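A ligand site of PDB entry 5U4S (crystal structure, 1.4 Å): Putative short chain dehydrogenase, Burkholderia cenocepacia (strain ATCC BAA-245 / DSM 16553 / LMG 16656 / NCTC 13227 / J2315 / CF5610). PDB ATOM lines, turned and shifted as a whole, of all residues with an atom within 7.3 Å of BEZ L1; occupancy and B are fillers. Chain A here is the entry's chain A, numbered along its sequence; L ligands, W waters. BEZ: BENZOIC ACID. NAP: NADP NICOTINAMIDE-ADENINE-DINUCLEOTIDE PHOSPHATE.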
ATOM      1  N   LEU A  90       7.923 -12.950 -12.754  1.00  0.00           N
ATOM      2  CA  LEU A  90       8.739 -13.239 -11.587  1.00  0.00           C
ATOM      3  C   LEU A  90       7.853 -13.409 -10.359  1.00  0.00           C
ATOM      4  O   LEU A  90       7.029 -12.537 -10.064  1.00  0.00           O
ATOM      5  CB  LEU A  90       9.703 -12.067 -11.323  1.00  0.00           C
ATOM      6  CG  LEU A  90      10.504 -12.092 -10.002  1.00  0.00           C
ATOM      7  CD1 LEU A  90      11.507 -13.268 -10.017  1.00  0.00           C
ATOM      8  CD2 LEU A  90      11.227 -10.787  -9.759  1.00  0.00           C
ATOM      9  N   ASN A  91       8.051 -14.497  -9.615  1.00  0.00           N
ATOM     10  CA  ASN A  91       7.344 -14.730  -8.352  1.00  0.00           C
ATOM     11  C   ASN A  91       8.390 -14.997  -7.274  1.00  0.00           C
ATOM     12  O   ASN A  91       9.007 -16.078  -7.236  1.00  0.00           O
ATOM     13  CB  ASN A  91       6.358 -15.909  -8.492  1.00  0.00           C
ATOM     14  CG  ASN A  91       5.547 -16.140  -7.214  1.00  0.00           C
ATOM     15  OD1 ASN A  91       5.826 -15.551  -6.163  1.00  0.00           O
ATOM     16  ND2 ASN A  91       4.538 -17.010  -7.296  1.00  0.00           N
ATOM     17  N   MET A  93       7.680 -15.217  -4.064  1.00  0.00           N
ATOM     18  CA  MET A  93       7.041 -16.021  -3.020  1.00  0.00           C
ATOM     19  C   MET A  93       7.367 -15.513  -1.625  1.00  0.00           C
ATOM     20  O   MET A  93       7.873 -16.225  -0.763  1.00  0.00           O
ATOM     21  CB  MET A  93       7.336 -17.517  -3.186  1.00  0.00           C
ATOM     22  CG  MET A  93       6.801 -18.030  -4.515  1.00  0.00           C
ATOM     23  SD  MET A  93       6.828 -19.805  -4.737  1.00  0.00           S
ATOM     24  CE  MET A  93       6.141 -19.907  -6.383  1.00  0.00           C
ATOM     25  N   LEU A 138      -0.967 -13.453 -16.849  1.00  0.00           N
ATOM     26  CA  LEU A 138      -1.003 -12.868 -15.508  1.00  0.00           C
ATOM     27  C   LEU A 138      -0.961 -13.986 -14.485  1.00  0.00           C
ATOM     28  O   LEU A 138       0.006 -14.746 -14.465  1.00  0.00           O
ATOM     29  CB  LEU A 138      -2.207 -11.922 -15.374  1.00  0.00           C
ATOM     30  CG  LEU A 138      -2.183 -10.808 -16.439  1.00  0.00           C
ATOM     31  CD1 LEU A 138      -3.307  -9.836 -16.143  1.00  0.00           C
ATOM     32  CD2 LEU A 138      -0.857 -10.057 -16.496  1.00  0.00           C
ATOM     33  N   SER A 139      -1.979 -14.104 -13.626  1.00  0.00           N
ATOM     34  CA  SER A 139      -2.080 -15.148 -12.613  1.00  0.00           C
ATOM     35  C   SER A 139      -3.464 -15.019 -12.014  1.00  0.00           C
ATOM     36  O   SER A 139      -4.013 -13.921 -11.952  1.00  0.00           O
ATOM     37  CB  SER A 139      -1.052 -14.929 -11.485  1.00  0.00           C
ATOM     38  OG  SER A 139      -1.292 -15.843 -10.403  1.00  0.00           O
ATOM     39  N   ILE A 140      -4.012 -16.146 -11.558  1.00  0.00           N
ATOM     40  CA  ILE A 140      -5.236 -16.066 -10.764  1.00  0.00           C
ATOM     41  C   ILE A 140      -5.022 -15.163  -9.549  1.00  0.00           C
ATOM     42  O   ILE A 140      -5.969 -14.560  -9.050  1.00  0.00           O
ATOM     43  CB  ILE A 140      -5.756 -17.472 -10.372  1.00  0.00           C
ATOM     44  CG1 ILE A 140      -7.125 -17.376  -9.677  1.00  0.00           C
ATOM     45  CG2 ILE A 140      -4.782 -18.205  -9.488  1.00  0.00           C
ATOM     46  CD1 ILE A 140      -8.210 -16.725 -10.545  1.00  0.00           C
ATOM     47  N   LEU A 141      -3.777 -15.066  -9.057  1.00  0.00           N
ATOM     48  CA  LEU A 141      -3.519 -14.216  -7.894  1.00  0.00           C
ATOM     49  C   LEU A 141      -3.621 -12.723  -8.202  1.00  0.00           C
ATOM     50  O   LEU A 141      -3.617 -11.910  -7.276  1.00  0.00           O
ATOM     51  CB  LEU A 141      -2.195 -14.568  -7.212  1.00  0.00           C
ATOM     52  CG  LEU A 141      -2.124 -16.048  -6.817  1.00  0.00           C
ATOM     53  CD1 LEU A 141      -0.799 -16.312  -6.086  1.00  0.00           C
ATOM     54  CD2 LEU A 141      -3.330 -16.528  -5.968  1.00  0.00           C
ATOM     55  N   ALA A 142      -3.809 -12.347  -9.469  1.00  0.00           N
ATOM     56  CA  ALA A 142      -4.211 -10.968  -9.758  1.00  0.00           C
ATOM     57  C   ALA A 142      -5.541 -10.622  -9.118  1.00  0.00           C
ATOM     58  O   ALA A 142      -5.813  -9.444  -8.901  1.00  0.00           O
ATOM     59  CB  ALA A 142      -4.369 -10.765 -11.265  1.00  0.00           C
ATOM     60  N   LEU A 146      -2.666 -14.771  -2.041  1.00  0.00           N
ATOM     61  CA  LEU A 146      -2.303 -15.809  -1.088  1.00  0.00           C
ATOM     62  C   LEU A 146      -1.295 -15.197  -0.146  1.00  0.00           C
ATOM     63  O   LEU A 146      -0.362 -14.529  -0.606  1.00  0.00           O
ATOM     64  CB  LEU A 146      -1.674 -17.009  -1.770  1.00  0.00           C
ATOM     65  CG  LEU A 146      -2.537 -17.875  -2.672  1.00  0.00           C
ATOM     66  CD1 LEU A 146      -1.705 -19.075  -3.156  1.00  0.00           C
ATOM     67  CD2 LEU A 146      -3.810 -18.344  -1.972  1.00  0.00           C
ATOM     68  N   MET A 149       2.472 -15.209  -0.857  1.00  0.00           N
ATOM     69  CA  MET A 149       2.865 -14.681  -2.165  1.00  0.00           C
ATOM     70  C   MET A 149       2.128 -13.380  -2.439  1.00  0.00           C
ATOM     71  O   MET A 149       1.796 -13.081  -3.590  1.00  0.00           O
ATOM     72  CB  MET A 149       2.533 -15.652  -3.315  1.00  0.00           C
ATOM     73  CG  MET A 149       2.949 -17.057  -3.122  1.00  0.00           C
ATOM     74  SD  MET A 149       2.334 -17.973  -4.570  1.00  0.00           S
ATOM     75  CE  MET A 149       2.819 -19.603  -4.031  1.00  0.00           C
ATOM     76  N   LEU A 152       3.593 -10.913  -5.036  1.00  0.00           N
ATOM     77  CA  LEU A 152       3.377 -11.359  -6.411  1.00  0.00           C
ATOM     78  C   LEU A 152       1.947 -11.026  -6.831  1.00  0.00           C
ATOM     79  O   LEU A 152       1.710 -10.461  -7.906  1.00  0.00           O
ATOM     80  CB  LEU A 152       3.618 -12.868  -6.529  1.00  0.00           C
ATOM     81  CG  LEU A 152       3.235 -13.592  -7.851  1.00  0.00           C
ATOM     82  CD1 LEU A 152       1.744 -13.904  -8.014  1.00  0.00           C
ATOM     83  CD2 LEU A 152       3.810 -12.890  -9.107  1.00  0.00           C
ATOM     84  N   SER A 153       0.986 -11.338  -5.941  1.00  0.00           N
ATOM     85  CA  SER A 153      -0.411 -11.052  -6.216  1.00  0.00           C
ATOM     86  C   SER A 153      -0.620  -9.578  -6.545  1.00  0.00           C
ATOM     87  O   SER A 153      -1.268  -9.240  -7.544  1.00  0.00           O
ATOM     88  CB  SER A 153      -1.191 -11.466  -4.967  1.00  0.00           C
ATOM     89  OG  SER A 153      -2.560 -11.105  -5.039  1.00  0.00           O
ATOM     90  N   LYS A 156       0.584  -8.669 -10.033  1.00  0.00           N
ATOM     91  CA  LYS A 156      -0.274  -9.183 -11.096  1.00  0.00           C
ATOM     92  C   LYS A 156      -1.619  -8.465 -11.139  1.00  0.00           C
ATOM     93  O   LYS A 156      -2.178  -8.311 -12.230  1.00  0.00           O
ATOM     94  CB  LYS A 156      -0.412 -10.707 -10.971  1.00  0.00           C
ATOM     95  CG  LYS A 156       0.892 -11.489 -11.231  1.00  0.00           C
ATOM     96  CD  LYS A 156       1.193 -11.571 -12.716  1.00  0.00           C
ATOM     97  CE  LYS A 156       2.324 -12.590 -12.924  1.00  0.00           C
ATOM     98  NZ  LYS A 156       2.647 -12.839 -14.380  1.00  0.00           N
ATOM     99  N   PRO A 182      -3.676 -18.034 -14.954  1.00  0.00           N
ATOM    100  CA  PRO A 182      -3.487 -19.433 -14.544  1.00  0.00           C
ATOM    101  C   PRO A 182      -3.303 -19.596 -13.054  1.00  0.00           C
ATOM    102  O   PRO A 182      -2.853 -18.698 -12.338  1.00  0.00           O
ATOM    103  CB  PRO A 182      -2.146 -19.831 -15.220  1.00  0.00           C
ATOM    104  CG  PRO A 182      -1.728 -18.661 -16.044  1.00  0.00           C
ATOM    105  CD  PRO A 182      -2.470 -17.450 -15.559  1.00  0.00           C
ATOM    106  N   GLY A 183      -3.678 -20.796 -12.594  1.00  0.00           N
ATOM    107  CA  GLY A 183      -3.157 -21.332 -11.360  1.00  0.00           C
ATOM    108  C   GLY A 183      -1.806 -21.966 -11.602  1.00  0.00           C
ATOM    109  O   GLY A 183      -1.173 -21.729 -12.645  1.00  0.00           O
ATOM    110  N   PRO A 184      -1.343 -22.827 -10.694  1.00  0.00           N
ATOM    111  CA  PRO A 184       0.020 -23.359 -10.805  1.00  0.00           C
ATOM    112  C   PRO A 184       0.242 -24.144 -12.083  1.00  0.00           C
ATOM    113  O   PRO A 184      -0.600 -24.946 -12.496  1.00  0.00           O
ATOM    114  CB  PRO A 184       0.148 -24.256  -9.569  1.00  0.00           C
ATOM    115  CG  PRO A 184      -0.797 -23.601  -8.581  1.00  0.00           C
ATOM    116  CD  PRO A 184      -1.967 -23.167  -9.400  1.00  0.00           C
ATOM    117  N   ILE A 185       1.399 -23.891 -12.719  1.00  0.00           N
ATOM    118  CA  ILE A 185       1.851 -24.573 -13.919  1.00  0.00           C
ATOM    119  C   ILE A 185       3.168 -25.248 -13.577  1.00  0.00           C
ATOM    120  O   ILE A 185       3.972 -24.710 -12.802  1.00  0.00           O
ATOM    121  CB  ILE A 185       2.063 -23.558 -15.075  1.00  0.00           C
ATOM    122  CG1 ILE A 185       0.810 -22.707 -15.309  1.00  0.00           C
ATOM    123  CG2 ILE A 185       2.432 -24.275 -16.393  1.00  0.00           C
ATOM    124  CD1 ILE A 185       1.056 -21.488 -16.214  1.00  0.00           C
ATOM    125  N   MET A 189       9.262 -21.882 -11.967  1.00  0.00           N
ATOM    126  CA  MET A 189       8.690 -20.859 -11.090  1.00  0.00           C
ATOM    127  C   MET A 189       7.987 -21.478  -9.887  1.00  0.00           C
ATOM    128  O   MET A 189       8.055 -20.956  -8.765  1.00  0.00           O
ATOM    129  CB  MET A 189       7.705 -19.991 -11.867  1.00  0.00           C
ATOM    130  CG  MET A 189       7.019 -18.974 -10.964  1.00  0.00           C
ATOM    131  SD  MET A 189       5.987 -17.836 -11.876  1.00  0.00           S
ATOM    132  CE  MET A 189       7.258 -16.851 -12.711  1.00  0.00           C
ATOM    133  N   SER A 190       7.296 -22.605 -10.113  1.00  0.00           N
ATOM    134  CA  SER A 190       6.473 -23.248  -9.088  1.00  0.00           C
ATOM    135  C   SER A 190       7.112 -24.513  -8.513  1.00  0.00           C
ATOM    136  O   SER A 190       6.383 -25.359  -7.994  1.00  0.00           O
ATOM    137  CB  SER A 190       5.095 -23.562  -9.654  1.00  0.00           C
ATOM    138  OG  SER A 190       5.131 -24.678 -10.521  1.00  0.00           O
ATOM    139  N   VAL A 193       5.860 -24.939  -5.074  1.00  0.00           N
ATOM    140  CA  VAL A 193       4.426 -25.158  -4.951  1.00  0.00           C
ATOM    141  C   VAL A 193       4.166 -26.651  -5.063  1.00  0.00           C
ATOM    142  O   VAL A 193       4.647 -27.289  -6.019  1.00  0.00           O
ATOM    143  CB  VAL A 193       3.692 -24.385  -6.042  1.00  0.00           C
ATOM    144  CG1 VAL A 193       2.193 -24.579  -5.914  1.00  0.00           C
ATOM    145  CG2 VAL A 193       4.064 -22.917  -5.990  1.00  0.00           C
ATOM    146  N   MET A 223      -8.176 -24.806 -10.462  1.00  0.00           N
ATOM    147  CA  MET A 223      -8.024 -23.904  -9.330  1.00  0.00           C
ATOM    148  C   MET A 223      -8.451 -22.494  -9.715  1.00  0.00           C
ATOM    149  O   MET A 223      -9.187 -21.831  -8.992  1.00  0.00           O
ATOM    150  CB  MET A 223      -6.591 -23.866  -8.793  1.00  0.00           C
ATOM    151  CG  MET A 223      -6.424 -22.788  -7.676  1.00  0.00           C
ATOM    152  SD  MET A 223      -4.761 -22.216  -7.204  1.00  0.00           S
ATOM    153  CE  MET A 223      -4.075 -23.773  -6.644  1.00  0.00           C
ATOM    154  N   ILE A 227     -11.587 -20.338  -8.129  1.00  0.00           N
ATOM    155  CA  ILE A 227     -11.383 -19.070  -7.447  1.00  0.00           C
ATOM    156  C   ILE A 227     -12.202 -17.968  -8.108  1.00  0.00           C
ATOM    157  O   ILE A 227     -12.861 -17.180  -7.420  1.00  0.00           O
ATOM    158  CB  ILE A 227      -9.877 -18.728  -7.364  1.00  0.00           C
ATOM    159  CG1 ILE A 227      -9.211 -19.662  -6.363  1.00  0.00           C
ATOM    160  CG2 ILE A 227      -9.683 -17.270  -6.958  1.00  0.00           C
ATOM    161  CD1 ILE A 227      -7.699 -19.539  -6.311  1.00  0.00           C
HETATM  162  C   BEZ L   1       1.538 -17.889  -9.317  1.00  0.00           C
HETATM  163  O1  BEZ L   1       2.786 -18.118  -9.352  1.00  0.00           O
HETATM  164  O2  BEZ L   1       1.075 -16.925  -9.981  1.00  0.00           O
HETATM  165  C1  BEZ L   1       0.611 -18.762  -8.526  1.00  0.00           C
HETATM  166  C2  BEZ L   1      -0.746 -18.816  -8.795  1.00  0.00           C
HETATM  167  C3  BEZ L   1      -1.587 -19.627  -8.041  1.00  0.00           C
HETATM  168  C4  BEZ L   1      -1.040 -20.348  -6.981  1.00  0.00           C
HETATM  169  C5  BEZ L   1       0.328 -20.295  -6.721  1.00  0.00           C
HETATM  170  C6  BEZ L   1       1.165 -19.504  -7.502  1.00  0.00           C
HETATM  171  PA  NAP L   2       9.539 -19.897 -15.526  1.00  0.00           P
HETATM  172  O1A NAP L   2      10.242 -19.644 -14.256  1.00  0.00           O
HETATM  173  O2A NAP L   2       9.717 -21.279 -16.109  1.00  0.00           O
HETATM  174  O5B NAP L   2       9.950 -18.838 -16.613  1.00  0.00           O
HETATM  175  C5B NAP L   2       9.897 -17.435 -16.291  1.00  0.00           C
HETATM  176  C4B NAP L   2      10.399 -16.735 -17.526  1.00  0.00           C
HETATM  177  O4B NAP L   2      10.342 -15.301 -17.308  1.00  0.00           O
HETATM  178  C3B NAP L   2      11.850 -17.069 -17.890  1.00  0.00           C
HETATM  179  O3B NAP L   2      11.969 -17.207 -19.313  1.00  0.00           O
HETATM  180  C2B NAP L   2      12.587 -15.835 -17.394  1.00  0.00           C
HETATM  181  O2B NAP L   2      13.832 -15.544 -18.047  1.00  0.00           O
HETATM  182  C1B NAP L   2      11.569 -14.770 -17.748  1.00  0.00           C
HETATM  183  N9A NAP L   2      11.826 -13.480 -17.118  1.00  0.00           N
HETATM  184  C8A NAP L   2      11.819 -13.146 -15.786  1.00  0.00           C
HETATM  185  N7A NAP L   2      12.208 -11.915 -15.550  1.00  0.00           N
HETATM  186  C5A NAP L   2      12.474 -11.395 -16.800  1.00  0.00           C
HETATM  187  C6A NAP L   2      12.887 -10.123 -17.244  1.00  0.00           C
HETATM  188  N6A NAP L   2      13.209  -9.117 -16.430  1.00  0.00           N
HETATM  189  N1A NAP L   2      12.998  -9.932 -18.582  1.00  0.00           N
HETATM  190  C2A NAP L   2      12.751 -10.952 -19.402  1.00  0.00           C
HETATM  191  N3A NAP L   2      12.380 -12.200 -19.106  1.00  0.00           N
HETATM  192  C4A NAP L   2      12.244 -12.357 -17.781  1.00  0.00           C
HETATM  193  O3  NAP L   2       7.993 -19.620 -15.244  1.00  0.00           O
HETATM  194  PN  NAP L   2       6.686 -19.764 -16.152  1.00  0.00           P
HETATM  195  O1N NAP L   2       5.700 -20.552 -15.404  1.00  0.00           O
HETATM  196  O2N NAP L   2       7.061 -20.229 -17.508  1.00  0.00           O
HETATM  197  O5D NAP L   2       6.207 -18.233 -16.212  1.00  0.00           O
HETATM  198  C5D NAP L   2       5.493 -17.752 -17.376  1.00  0.00           C
HETATM  199  C4D NAP L   2       4.408 -16.810 -16.919  1.00  0.00           C
HETATM  200  O4D NAP L   2       3.336 -17.557 -16.279  1.00  0.00           O
HETATM  201  C3D NAP L   2       4.841 -15.732 -15.909  1.00  0.00           C
HETATM  202  O3D NAP L   2       4.259 -14.473 -16.244  1.00  0.00           O
HETATM  203  C2D NAP L   2       4.265 -16.260 -14.597  1.00  0.00           C
HETATM  204  O2D NAP L   2       4.067 -15.197 -13.666  1.00  0.00           O
HETATM  205  C1D NAP L   2       2.967 -16.874 -15.109  1.00  0.00           C
HETATM  206  N1N NAP L   2       2.355 -17.844 -14.172  1.00  0.00           N
HETATM  207  C2N NAP L   2       3.065 -18.939 -13.833  1.00  0.00           C
HETATM  208  C3N NAP L   2       2.571 -19.820 -12.892  1.00  0.00           C
HETATM  209  C7N NAP L   2       3.325 -21.058 -12.486  1.00  0.00           C
HETATM  210  O7N NAP L   2       4.379 -21.403 -13.115  1.00  0.00           O
HETATM  211  N7N NAP L   2       2.806 -21.781 -11.530  1.00  0.00           N
HETATM  212  C4N NAP L   2       1.323 -19.567 -12.318  1.00  0.00           C
HETATM  213  C5N NAP L   2       0.614 -18.445 -12.706  1.00  0.00           C
HETATM  214  C6N NAP L   2       1.143 -17.590 -13.645  1.00  0.00           C
HETATM  215  P2B NAP L   2      15.205 -16.299 -17.643  1.00  0.00           P
HETATM  216  O1X NAP L   2      15.089 -17.752 -18.029  1.00  0.00           O
HETATM  217  O2X NAP L   2      15.281 -16.173 -16.125  1.00  0.00           O
HETATM  218  O3X NAP L   2      16.230 -15.495 -18.390  1.00  0.00           O
HETATM  219  O   HOH W   1       3.270 -15.968 -11.248  1.00  0.00           O
HETATM  220  O   HOH W   2       4.184 -20.487  -9.089  1.00  0.00           O
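The backbone NH (N) of Met 93 is in hydrogen-bond range of the side-chain amide oxygen (OD1) of Asn 91 (2.8 Å).
The side-chain amide nitrogen of Asn 91 sits at hydrogen-bond distance from the side-chain sulfur of Met 149, at 3.6 Å.
The side-chain hydroxyl of Ser 139 is in hydrogen-bond range of the backbone NH of Leu 141, 2.9 Å away.
N of Ile 140 lies within hydrogen-bond range of O of Pro 182 (2.9 Å).
The backbone carbonyl oxygen of Leu 141 sits at hydrogen-bond distance from the side-chain hydroxyl of Ser 153, at 2.6 Å.
Residues that only touch BEZ L1: Met 149, Pro 184, Leu 152, Leu 141 and Ile 140.
Hydrophobic or aromatic side chains within 4 Å of BEZ L1: Ile 140, Leu 141, Met 149, Leu 152 and Pro 184.
Within 4 Å of BEZ L1: Asn 91, Ser 139, Ile 140, Leu 141, Met 149, Leu 152 and Pro 184.
Water W1 lies within hydrogen-bond range of an oxygen (O2D) of NAP L2, an oxygen (O2) of BEZ L1 and the side-chain sulfur (SD) of Met 189.
Water W2 bridges an oxygen (O1) of BEZ L1 (2.8 Å) and a nitrogen (N7N) of NAP L2 (3.1 Å).
The side-chain amino group of Lys 156 lies within hydrogen-bond range of an oxygen (O2D) of NAP L2.
The backbone carbonyl oxygen (O) of Ile 185 lies within hydrogen-bond range of a nitrogen (N7N) of NAP L2, 3.4 Å away.
An oxygen (O2) of BEZ L1 sits at hydrogen-bond distance from the side-chain hydroxyl (OG) of Ser 139.
The side-chain amide nitrogen (ND2) of Asn 91 is in hydrogen-bond range of an oxygen (O1) of BEZ L1 (2.9 Å).
An oxygen (O1A) of NAP L2 sits at hydrogen-bond distance from the backbone NH (N) of Met 189 (3.3 Å).
The side-chain sulfur of Met 189 lies close to an oxygen (O2D) of NAP L2, at 3.7 Å.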
